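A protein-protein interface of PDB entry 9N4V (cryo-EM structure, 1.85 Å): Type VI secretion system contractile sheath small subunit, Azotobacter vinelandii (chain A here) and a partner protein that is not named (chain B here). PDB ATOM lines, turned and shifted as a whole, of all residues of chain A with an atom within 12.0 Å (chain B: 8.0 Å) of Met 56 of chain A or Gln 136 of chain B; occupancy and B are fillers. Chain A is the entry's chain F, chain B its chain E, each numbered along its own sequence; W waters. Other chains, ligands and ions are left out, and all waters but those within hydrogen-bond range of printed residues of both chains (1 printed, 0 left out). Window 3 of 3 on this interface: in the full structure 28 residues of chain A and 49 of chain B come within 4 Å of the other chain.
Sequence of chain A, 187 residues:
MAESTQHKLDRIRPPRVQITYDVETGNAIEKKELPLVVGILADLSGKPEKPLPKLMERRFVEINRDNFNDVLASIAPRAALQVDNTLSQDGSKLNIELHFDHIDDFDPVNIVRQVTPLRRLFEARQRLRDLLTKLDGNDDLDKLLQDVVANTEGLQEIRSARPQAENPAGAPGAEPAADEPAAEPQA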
ATOM      1  N   LEU A  41       5.678 -28.226  21.807  1.00  0.00           N
ATOM      2  CA  LEU A  41       5.890 -27.989  23.232  1.00  0.00           C
ATOM      3  C   LEU A  41       6.483 -29.261  23.823  1.00  0.00           C
ATOM      4  O   LEU A  41       5.826 -30.305  23.837  1.00  0.00           O
ATOM      5  CB  LEU A  41       4.585 -27.619  23.935  1.00  0.00           C
ATOM      6  CG  LEU A  41       3.827 -26.373  23.487  1.00  0.00           C
ATOM      7  CD1 LEU A  41       2.867 -25.922  24.571  1.00  0.00           C
ATOM      8  CD2 LEU A  41       4.786 -25.268  23.156  1.00  0.00           C
ATOM      9  N   MET A  56       7.850 -16.174  29.796  1.00  0.00           N
ATOM     10  CA  MET A  56       7.812 -14.946  29.010  1.00  0.00           C
ATOM     11  C   MET A  56       9.102 -14.757  28.228  1.00  0.00           C
ATOM     12  O   MET A  56       9.098 -14.214  27.126  1.00  0.00           O
ATOM     13  CB  MET A  56       7.578 -13.735  29.912  1.00  0.00           C
ATOM     14  CG  MET A  56       6.559 -12.726  29.392  1.00  0.00           C
ATOM     15  SD  MET A  56       5.105 -13.438  28.599  1.00  0.00           S
ATOM     16  CE  MET A  56       3.948 -13.443  29.970  1.00  0.00           C
ATOM     17  N   GLU A  57      10.207 -15.211  28.815  1.00  0.00           N
ATOM     18  CA  GLU A  57      11.528 -14.955  28.258  1.00  0.00           C
ATOM     19  C   GLU A  57      11.904 -15.920  27.141  1.00  0.00           C
ATOM     20  O   GLU A  57      12.749 -15.579  26.309  1.00  0.00           O
ATOM     21  CB  GLU A  57      12.581 -15.015  29.371  1.00  0.00           C
ATOM     22  CG  GLU A  57      12.827 -16.406  29.955  1.00  0.00           C
ATOM     23  CD  GLU A  57      11.837 -16.796  31.046  1.00  0.00           C
ATOM     24  OE1 GLU A  57      10.727 -17.249  30.710  1.00  0.00           O
ATOM     25  OE2 GLU A  57      12.180 -16.665  32.243  1.00  0.00           O
ATOM     26  N   ARG A  58      11.305 -17.106  27.100  1.00  0.00           N
ATOM     27  CA  ARG A  58      11.646 -18.089  26.086  1.00  0.00           C
ATOM     28  C   ARG A  58      10.903 -17.786  24.789  1.00  0.00           C
ATOM     29  O   ARG A  58      10.093 -16.861  24.705  1.00  0.00           O
ATOM     30  CB  ARG A  58      11.342 -19.493  26.594  1.00  0.00           C
ATOM     31  CG  ARG A  58      11.955 -19.773  27.946  1.00  0.00           C
ATOM     32  CD  ARG A  58      11.681 -21.175  28.411  1.00  0.00           C
ATOM     33  NE  ARG A  58      11.751 -21.267  29.862  1.00  0.00           N
ATOM     34  CZ  ARG A  58      11.305 -22.294  30.568  1.00  0.00           C
ATOM     35  NH1 ARG A  58      10.759 -23.347  29.986  1.00  0.00           N
ATOM     36  NH2 ARG A  58      11.407 -22.262  31.893  1.00  0.00           N
ATOM     37  N   ARG A  59      11.179 -18.575  23.756  1.00  0.00           N
ATOM     38  CA  ARG A  59      10.579 -18.324  22.458  1.00  0.00           C
ATOM     39  C   ARG A  59      10.480 -19.626  21.679  1.00  0.00           C
ATOM     40  O   ARG A  59      11.123 -20.624  22.009  1.00  0.00           O
ATOM     41  CB  ARG A  59      11.376 -17.279  21.672  1.00  0.00           C
ATOM     42  CG  ARG A  59      12.777 -17.714  21.303  1.00  0.00           C
ATOM     43  CD  ARG A  59      13.558 -16.568  20.679  1.00  0.00           C
ATOM     44  NE  ARG A  59      14.561 -17.037  19.729  1.00  0.00           N
ATOM     45  CZ  ARG A  59      14.341 -17.219  18.433  1.00  0.00           C
ATOM     46  NH1 ARG A  59      13.156 -16.988  17.892  1.00  0.00           N
ATOM     47  NH2 ARG A  59      15.336 -17.643  17.660  1.00  0.00           N
ATOM     48  N   PHE A  60       9.644 -19.603  20.647  1.00  0.00           N
ATOM     49  CA  PHE A  60       9.518 -20.716  19.713  1.00  0.00           C
ATOM     50  C   PHE A  60      10.656 -20.621  18.709  1.00  0.00           C
ATOM     51  O   PHE A  60      10.600 -19.831  17.767  1.00  0.00           O
ATOM     52  CB  PHE A  60       8.169 -20.674  19.008  1.00  0.00           C
ATOM     53  CG  PHE A  60       7.055 -21.318  19.773  1.00  0.00           C
ATOM     54  CD1 PHE A  60       6.798 -22.672  19.640  1.00  0.00           C
ATOM     55  CD2 PHE A  60       6.244 -20.566  20.606  1.00  0.00           C
ATOM     56  CE1 PHE A  60       5.761 -23.264  20.332  1.00  0.00           C
ATOM     57  CE2 PHE A  60       5.210 -21.154  21.299  1.00  0.00           C
ATOM     58  CZ  PHE A  60       4.967 -22.502  21.161  1.00  0.00           C
ATOM     59  N   VAL A  61      11.694 -21.423  18.900  1.00  0.00           N
ATOM     60  CA  VAL A  61      12.857 -21.394  18.022  1.00  0.00           C
ATOM     61  C   VAL A  61      12.616 -22.334  16.847  1.00  0.00           C
ATOM     62  O   VAL A  61      12.200 -23.484  17.030  1.00  0.00           O
ATOM     63  CB  VAL A  61      14.139 -21.760  18.792  1.00  0.00           C
ATOM     64  CG1 VAL A  61      14.363 -20.776  19.935  1.00  0.00           C
ATOM     65  CG2 VAL A  61      14.077 -23.173  19.332  1.00  0.00           C
ATOM     66  N   LEU B 117       9.230 -24.849  21.472  1.00  0.00           N
ATOM     67  CA  LEU B 117       9.252 -24.153  22.752  1.00  0.00           C
ATOM     68  C   LEU B 117       9.604 -25.155  23.841  1.00  0.00           C
ATOM     69  O   LEU B 117       8.840 -26.086  24.101  1.00  0.00           O
ATOM     70  CB  LEU B 117       7.907 -23.488  23.051  1.00  0.00           C
ATOM     71  CG  LEU B 117       7.834 -22.779  24.407  1.00  0.00           C
ATOM     72  CD1 LEU B 117       8.751 -21.574  24.413  1.00  0.00           C
ATOM     73  CD2 LEU B 117       6.407 -22.376  24.752  1.00  0.00           C
ATOM     74  N   ASP B 127       1.992 -21.095  34.255  1.00  0.00           N
ATOM     75  CA  ASP B 127       1.789 -19.937  33.392  1.00  0.00           C
ATOM     76  C   ASP B 127       0.312 -19.732  33.089  1.00  0.00           C
ATOM     77  O   ASP B 127      -0.187 -18.603  33.132  1.00  0.00           O
ATOM     78  CB  ASP B 127       2.586 -20.103  32.098  1.00  0.00           C
ATOM     79  CG  ASP B 127       2.156 -19.130  31.013  1.00  0.00           C
ATOM     80  OD1 ASP B 127       2.272 -17.905  31.226  1.00  0.00           O
ATOM     81  OD2 ASP B 127       1.714 -19.589  29.941  1.00  0.00           O
ATOM     82  N   LEU B 128      -0.410 -20.813  32.800  1.00  0.00           N
ATOM     83  CA  LEU B 128      -1.812 -20.673  32.430  1.00  0.00           C
ATOM     84  C   LEU B 128      -2.684 -20.349  33.637  1.00  0.00           C
ATOM     85  O   LEU B 128      -3.630 -19.565  33.527  1.00  0.00           O
ATOM     86  CB  LEU B 128      -2.291 -21.941  31.730  1.00  0.00           C
ATOM     87  CG  LEU B 128      -1.718 -22.061  30.320  1.00  0.00           C
ATOM     88  CD1 LEU B 128      -1.903 -23.461  29.768  1.00  0.00           C
ATOM     89  CD2 LEU B 128      -2.355 -21.020  29.412  1.00  0.00           C
ATOM     90  N   LYS B 130      -1.750 -18.829  36.557  1.00  0.00           N
ATOM     91  CA  LYS B 130      -1.410 -17.603  37.267  1.00  0.00           C
ATOM     92  C   LYS B 130      -1.623 -16.345  36.437  1.00  0.00           C
ATOM     93  O   LYS B 130      -1.447 -15.243  36.961  1.00  0.00           O
ATOM     94  CB  LYS B 130       0.043 -17.652  37.748  1.00  0.00           C
ATOM     95  CG  LYS B 130       0.244 -18.279  39.129  1.00  0.00           C
ATOM     96  CD  LYS B 130      -0.891 -19.223  39.517  1.00  0.00           C
ATOM     97  CE  LYS B 130      -0.874 -19.544  41.000  1.00  0.00           C
ATOM     98  NZ  LYS B 130      -2.061 -20.350  41.400  1.00  0.00           N
ATOM     99  N   ALA B 131      -1.978 -16.479  35.163  1.00  0.00           N
ATOM    100  CA  ALA B 131      -2.217 -15.306  34.335  1.00  0.00           C
ATOM    101  C   ALA B 131      -3.358 -14.480  34.915  1.00  0.00           C
ATOM    102  O   ALA B 131      -4.380 -15.020  35.344  1.00  0.00           O
ATOM    103  CB  ALA B 131      -2.539 -15.724  32.902  1.00  0.00           C
ATOM    104  N   VAL B 132      -3.168 -13.161  34.943  1.00  0.00           N
ATOM    105  CA  VAL B 132      -4.195 -12.280  35.493  1.00  0.00           C
ATOM    106  C   VAL B 132      -5.469 -12.368  34.661  1.00  0.00           C
ATOM    107  O   VAL B 132      -6.582 -12.330  35.196  1.00  0.00           O
ATOM    108  CB  VAL B 132      -3.663 -10.837  35.600  1.00  0.00           C
ATOM    109  CG1 VAL B 132      -3.025 -10.399  34.300  1.00  0.00           C
ATOM    110  CG2 VAL B 132      -4.769  -9.880  36.001  1.00  0.00           C
ATOM    111  N   GLU B 133      -5.326 -12.501  33.344  1.00  0.00           N
ATOM    112  CA  GLU B 133      -6.445 -12.712  32.436  1.00  0.00           C
ATOM    113  C   GLU B 133      -6.023 -13.736  31.392  1.00  0.00           C
ATOM    114  O   GLU B 133      -4.835 -13.994  31.199  1.00  0.00           O
ATOM    115  CB  GLU B 133      -6.896 -11.404  31.763  1.00  0.00           C
ATOM    116  CG  GLU B 133      -8.358 -11.401  31.318  1.00  0.00           C
ATOM    117  CD  GLU B 133      -8.834 -10.039  30.827  1.00  0.00           C
ATOM    118  OE1 GLU B 133      -7.994  -9.139  30.628  1.00  0.00           O
ATOM    119  OE2 GLU B 133     -10.057  -9.873  30.630  1.00  0.00           O
ATOM    120  N   PHE B 134      -7.014 -14.322  30.714  1.00  0.00           N
ATOM    121  CA  PHE B 134      -6.726 -15.435  29.813  1.00  0.00           C
ATOM    122  C   PHE B 134      -5.782 -15.034  28.686  1.00  0.00           C
ATOM    123  O   PHE B 134      -5.024 -15.873  28.192  1.00  0.00           O
ATOM    124  CB  PHE B 134      -8.027 -16.017  29.246  1.00  0.00           C
ATOM    125  CG  PHE B 134      -8.645 -15.196  28.150  1.00  0.00           C
ATOM    126  CD1 PHE B 134      -8.304 -15.410  26.823  1.00  0.00           C
ATOM    127  CD2 PHE B 134      -9.586 -14.226  28.444  1.00  0.00           C
ATOM    128  CE1 PHE B 134      -8.872 -14.659  25.822  1.00  0.00           C
ATOM    129  CE2 PHE B 134     -10.160 -13.475  27.443  1.00  0.00           C
ATOM    130  CZ  PHE B 134      -9.802 -13.693  26.131  1.00  0.00           C
ATOM    131  N   ASP B 135      -5.806 -13.772  28.267  1.00  0.00           N
ATOM    132  CA  ASP B 135      -4.959 -13.322  27.172  1.00  0.00           C
ATOM    133  C   ASP B 135      -3.608 -12.798  27.642  1.00  0.00           C
ATOM    134  O   ASP B 135      -2.856 -12.250  26.834  1.00  0.00           O
ATOM    135  CB  ASP B 135      -5.676 -12.253  26.341  1.00  0.00           C
ATOM    136  CG  ASP B 135      -6.089 -11.046  27.160  1.00  0.00           C
ATOM    137  OD1 ASP B 135      -5.870 -11.037  28.385  1.00  0.00           O
ATOM    138  OD2 ASP B 135      -6.641 -10.098  26.567  1.00  0.00           O
ATOM    139  N   GLN B 136      -3.289 -12.946  28.924  1.00  0.00           N
ATOM    140  CA  GLN B 136      -2.051 -12.421  29.479  1.00  0.00           C
ATOM    141  C   GLN B 136      -0.985 -13.486  29.693  1.00  0.00           C
ATOM    142  O   GLN B 136       0.167 -13.136  29.958  1.00  0.00           O
ATOM    143  CB  GLN B 136      -2.334 -11.706  30.804  1.00  0.00           C
ATOM    144  CG  GLN B 136      -3.236 -10.494  30.654  1.00  0.00           C
ATOM    145  CD  GLN B 136      -2.711  -9.507  29.634  1.00  0.00           C
ATOM    146  OE1 GLN B 136      -1.616  -8.974  29.782  1.00  0.00           O
ATOM    147  NE2 GLN B 136      -3.490  -9.262  28.591  1.00  0.00           N
ATOM    148  N   SER B 137      -1.334 -14.763  29.576  1.00  0.00           N
ATOM    149  CA  SER B 137      -0.365 -15.827  29.790  1.00  0.00           C
ATOM    150  C   SER B 137       0.709 -15.803  28.708  1.00  0.00           C
ATOM    151  O   SER B 137       0.485 -15.337  27.588  1.00  0.00           O
ATOM    152  CB  SER B 137      -1.061 -17.186  29.809  1.00  0.00           C
ATOM    153  OG  SER B 137      -1.365 -17.626  28.498  1.00  0.00           O
ATOM    154  N   ALA B 138       1.893 -16.304  29.059  1.00  0.00           N
ATOM    155  CA  ALA B 138       2.979 -16.366  28.088  1.00  0.00           C
ATOM    156  C   ALA B 138       2.583 -17.200  26.880  1.00  0.00           C
ATOM    157  O   ALA B 138       2.894 -16.845  25.738  1.00  0.00           O
ATOM    158  CB  ALA B 138       4.238 -16.935  28.740  1.00  0.00           C
ATOM    159  N   LEU B 139       1.887 -18.312  27.116  1.00  0.00           N
ATOM    160  CA  LEU B 139       1.455 -19.152  26.007  1.00  0.00           C
ATOM    161  C   LEU B 139       0.501 -18.409  25.082  1.00  0.00           C
ATOM    162  O   LEU B 139       0.630 -18.494  23.857  1.00  0.00           O
ATOM    163  CB  LEU B 139       0.808 -20.425  26.534  1.00  0.00           C
ATOM    164  CG  LEU B 139       1.093 -21.625  25.635  1.00  0.00           C
ATOM    165  CD1 LEU B 139       2.588 -21.899  25.567  1.00  0.00           C
ATOM    166  CD2 LEU B 139       0.345 -22.834  26.120  1.00  0.00           C
ATOM    167  N   PHE B 140      -0.466 -17.679  25.643  1.00  0.00           N
ATOM    168  CA  PHE B 140      -1.375 -16.921  24.792  1.00  0.00           C
ATOM    169  C   PHE B 140      -0.615 -15.886  23.976  1.00  0.00           C
ATOM    170  O   PHE B 140      -0.811 -15.782  22.765  1.00  0.00           O
ATOM    171  CB  PHE B 140      -2.476 -16.244  25.611  1.00  0.00           C
ATOM    172  CG  PHE B 140      -3.547 -15.607  24.760  1.00  0.00           C
ATOM    173  CD1 PHE B 140      -3.387 -14.327  24.253  1.00  0.00           C
ATOM    174  CD2 PHE B 140      -4.700 -16.302  24.443  1.00  0.00           C
ATOM    175  CE1 PHE B 140      -4.364 -13.748  23.463  1.00  0.00           C
ATOM    176  CE2 PHE B 140      -5.680 -15.729  23.658  1.00  0.00           C
ATOM    177  CZ  PHE B 140      -5.509 -14.451  23.164  1.00  0.00           C
ATOM    178  N   LYS B 141       0.276 -15.128  24.616  1.00  0.00           N
ATOM    179  CA  LYS B 141       1.050 -14.144  23.867  1.00  0.00           C
ATOM    180  C   LYS B 141       1.790 -14.807  22.713  1.00  0.00           C
ATOM    181  O   LYS B 141       1.546 -14.480  21.548  1.00  0.00           O
ATOM    182  CB  LYS B 141       2.020 -13.414  24.795  1.00  0.00           C
ATOM    183  CG  LYS B 141       1.338 -12.618  25.896  1.00  0.00           C
ATOM    184  CD  LYS B 141       1.019 -11.209  25.439  1.00  0.00           C
ATOM    185  CE  LYS B 141       0.357 -10.397  26.539  1.00  0.00           C
ATOM    186  NZ  LYS B 141       0.862 -10.793  27.879  1.00  0.00           N
ATOM    187  N   LYS B 142       2.567 -15.850  23.013  1.00  0.00           N
ATOM    188  CA  LYS B 142       3.441 -16.453  22.012  1.00  0.00           C
ATOM    189  C   LYS B 142       2.667 -17.152  20.899  1.00  0.00           C
ATOM    190  O   LYS B 142       3.110 -17.142  19.747  1.00  0.00           O
ATOM    191  CB  LYS B 142       4.402 -17.433  22.685  1.00  0.00           C
ATOM    192  CG  LYS B 142       5.457 -16.756  23.542  1.00  0.00           C
ATOM    193  CD  LYS B 142       6.286 -17.759  24.324  1.00  0.00           C
ATOM    194  CE  LYS B 142       6.955 -17.096  25.521  1.00  0.00           C
ATOM    195  NZ  LYS B 142       7.583 -15.800  25.157  1.00  0.00           N
ATOM    196  N   GLU B 145      -0.907 -13.938  19.993  1.00  0.00           N
ATOM    197  CA  GLU B 145      -0.646 -12.540  19.671  1.00  0.00           C
ATOM    198  C   GLU B 145       0.522 -12.397  18.709  1.00  0.00           C
ATOM    199  O   GLU B 145       0.441 -11.642  17.735  1.00  0.00           O
ATOM    200  CB  GLU B 145      -0.385 -11.740  20.948  1.00  0.00           C
ATOM    201  CG  GLU B 145      -1.549 -11.705  21.925  1.00  0.00           C
ATOM    202  CD  GLU B 145      -2.566 -10.625  21.594  1.00  0.00           C
ATOM    203  OE1 GLU B 145      -2.775 -10.336  20.401  1.00  0.00           O
ATOM    204  OE2 GLU B 145      -3.159 -10.062  22.532  1.00  0.00           O
ATOM    205  N   GLU B 146       1.608 -13.128  18.951  1.00  0.00           N
ATOM    206  CA  GLU B 146       2.832 -12.884  18.201  1.00  0.00           C
ATOM    207  C   GLU B 146       2.732 -13.368  16.759  1.00  0.00           C
ATOM    208  O   GLU B 146       3.449 -12.858  15.893  1.00  0.00           O
ATOM    209  CB  GLU B 146       4.015 -13.533  18.917  1.00  0.00           C
ATOM    210  CG  GLU B 146       4.583 -12.647  20.015  1.00  0.00           C
ATOM    211  CD  GLU B 146       5.498 -13.383  20.970  1.00  0.00           C
ATOM    212  OE1 GLU B 146       6.209 -14.307  20.531  1.00  0.00           O
ATOM    213  OE2 GLU B 146       5.505 -13.029  22.165  1.00  0.00           O
HETATM  214  O   HOH W   1       8.247 -17.127  20.272  1.00  0.00           O
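The side-chain amino group (NZ) of Lys 142 of chain B sits at hydrogen-bond distance from the backbone carbonyl oxygen (O) of Met 56 of chain A, at 2.9 Å. The side-chain amino group of Lys 142 of chain B lies within hydrogen-bond range of the backbone carbonyl oxygen of Arg 58 of chain A, 2.8 Å away.
The side-chain carboxylate (OD1) of Asp 127 of chain B lies within hydrogen-bond range of the backbone NH (N) of Ala 138 of chain B. The side-chain amide nitrogen (NE2) of Gln 136 of chain B sits at hydrogen-bond distance from the side-chain carboxylate (OD1) of Asp 135 of chain B (3.0 Å). The side-chain amino group of Lys 141 of chain B sits at hydrogen-bond distance from the backbone carbonyl oxygen of Gln 136 of chain B.
Among the printed residues, merely in contact across the chains: Leu 41 of chain A with Leu 117 of chain B, Met 56 of chain A with Gln 136 of chain B, Met 56 of chain A with Ala 138 of chain B, Arg 58 of chain A with Leu 117 of chain B, Arg 59 of chain A with Leu 117 of chain B and Phe 60 of chain A with Leu 117 of chain B.
Of the printed residues of chain B, Leu 41 of chain A touches Leu 117. Of the printed residues of chain B, Met 56 of chain A touches Gln 136 (3.8 Å), Ala 138 (3.6 Å) and Lys 142 (2.9 Å). Of the printed residues of chain B, Arg 58 of chain A touches Leu 117 and Lys 142. Printed residues of chain B within 4 Å of Phe 60 of chain A: Leu 117. No residue of chain A comes within 4 Å of Val 132 of chain B. Glu 133 of chain B touches none of the printed residues of chain A. No residue of chain A comes within 4 Å of Phe 134 of chain B. No residue of chain A comes within 4 Å of Asp 135 of chain B. Of chain A, only Met 56 comes within 4 Å of Ala 138 of chain B. No residue of chain A comes within 4 Å of Phe 140 of chain B. The nearest residue of chain B that does not touch Met 56 of chain A is Ser 137 of chain B (4.2 Å). The nearest residue of chain A that does not touch Gln 136 of chain B is Glu 57 of chain A (10.3 Å). The nearest printed residue of chain B that does not touch Arg 59 of chain A is Lys 142 of chain B (4.7 Å).
Hydrophobic or aromatic side chains of chain B that line the printed part of chain A: Leu 117 and Ala 138. Hydrophobic or aromatic side chains of chain A within 4 Å of the printed part of chain B: Leu 41, Met 56 and Phe 60. Among the printed residues, no Asp or Glu carboxylate lies within 4 Å of a Lys or Arg side-chain nitrogen of the other chain.
Water W1 lies within hydrogen-bond range of N of Phe 60 of chain A (2.9 Å) and OE1 of Glu 146 of chain B (3.5 Å).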
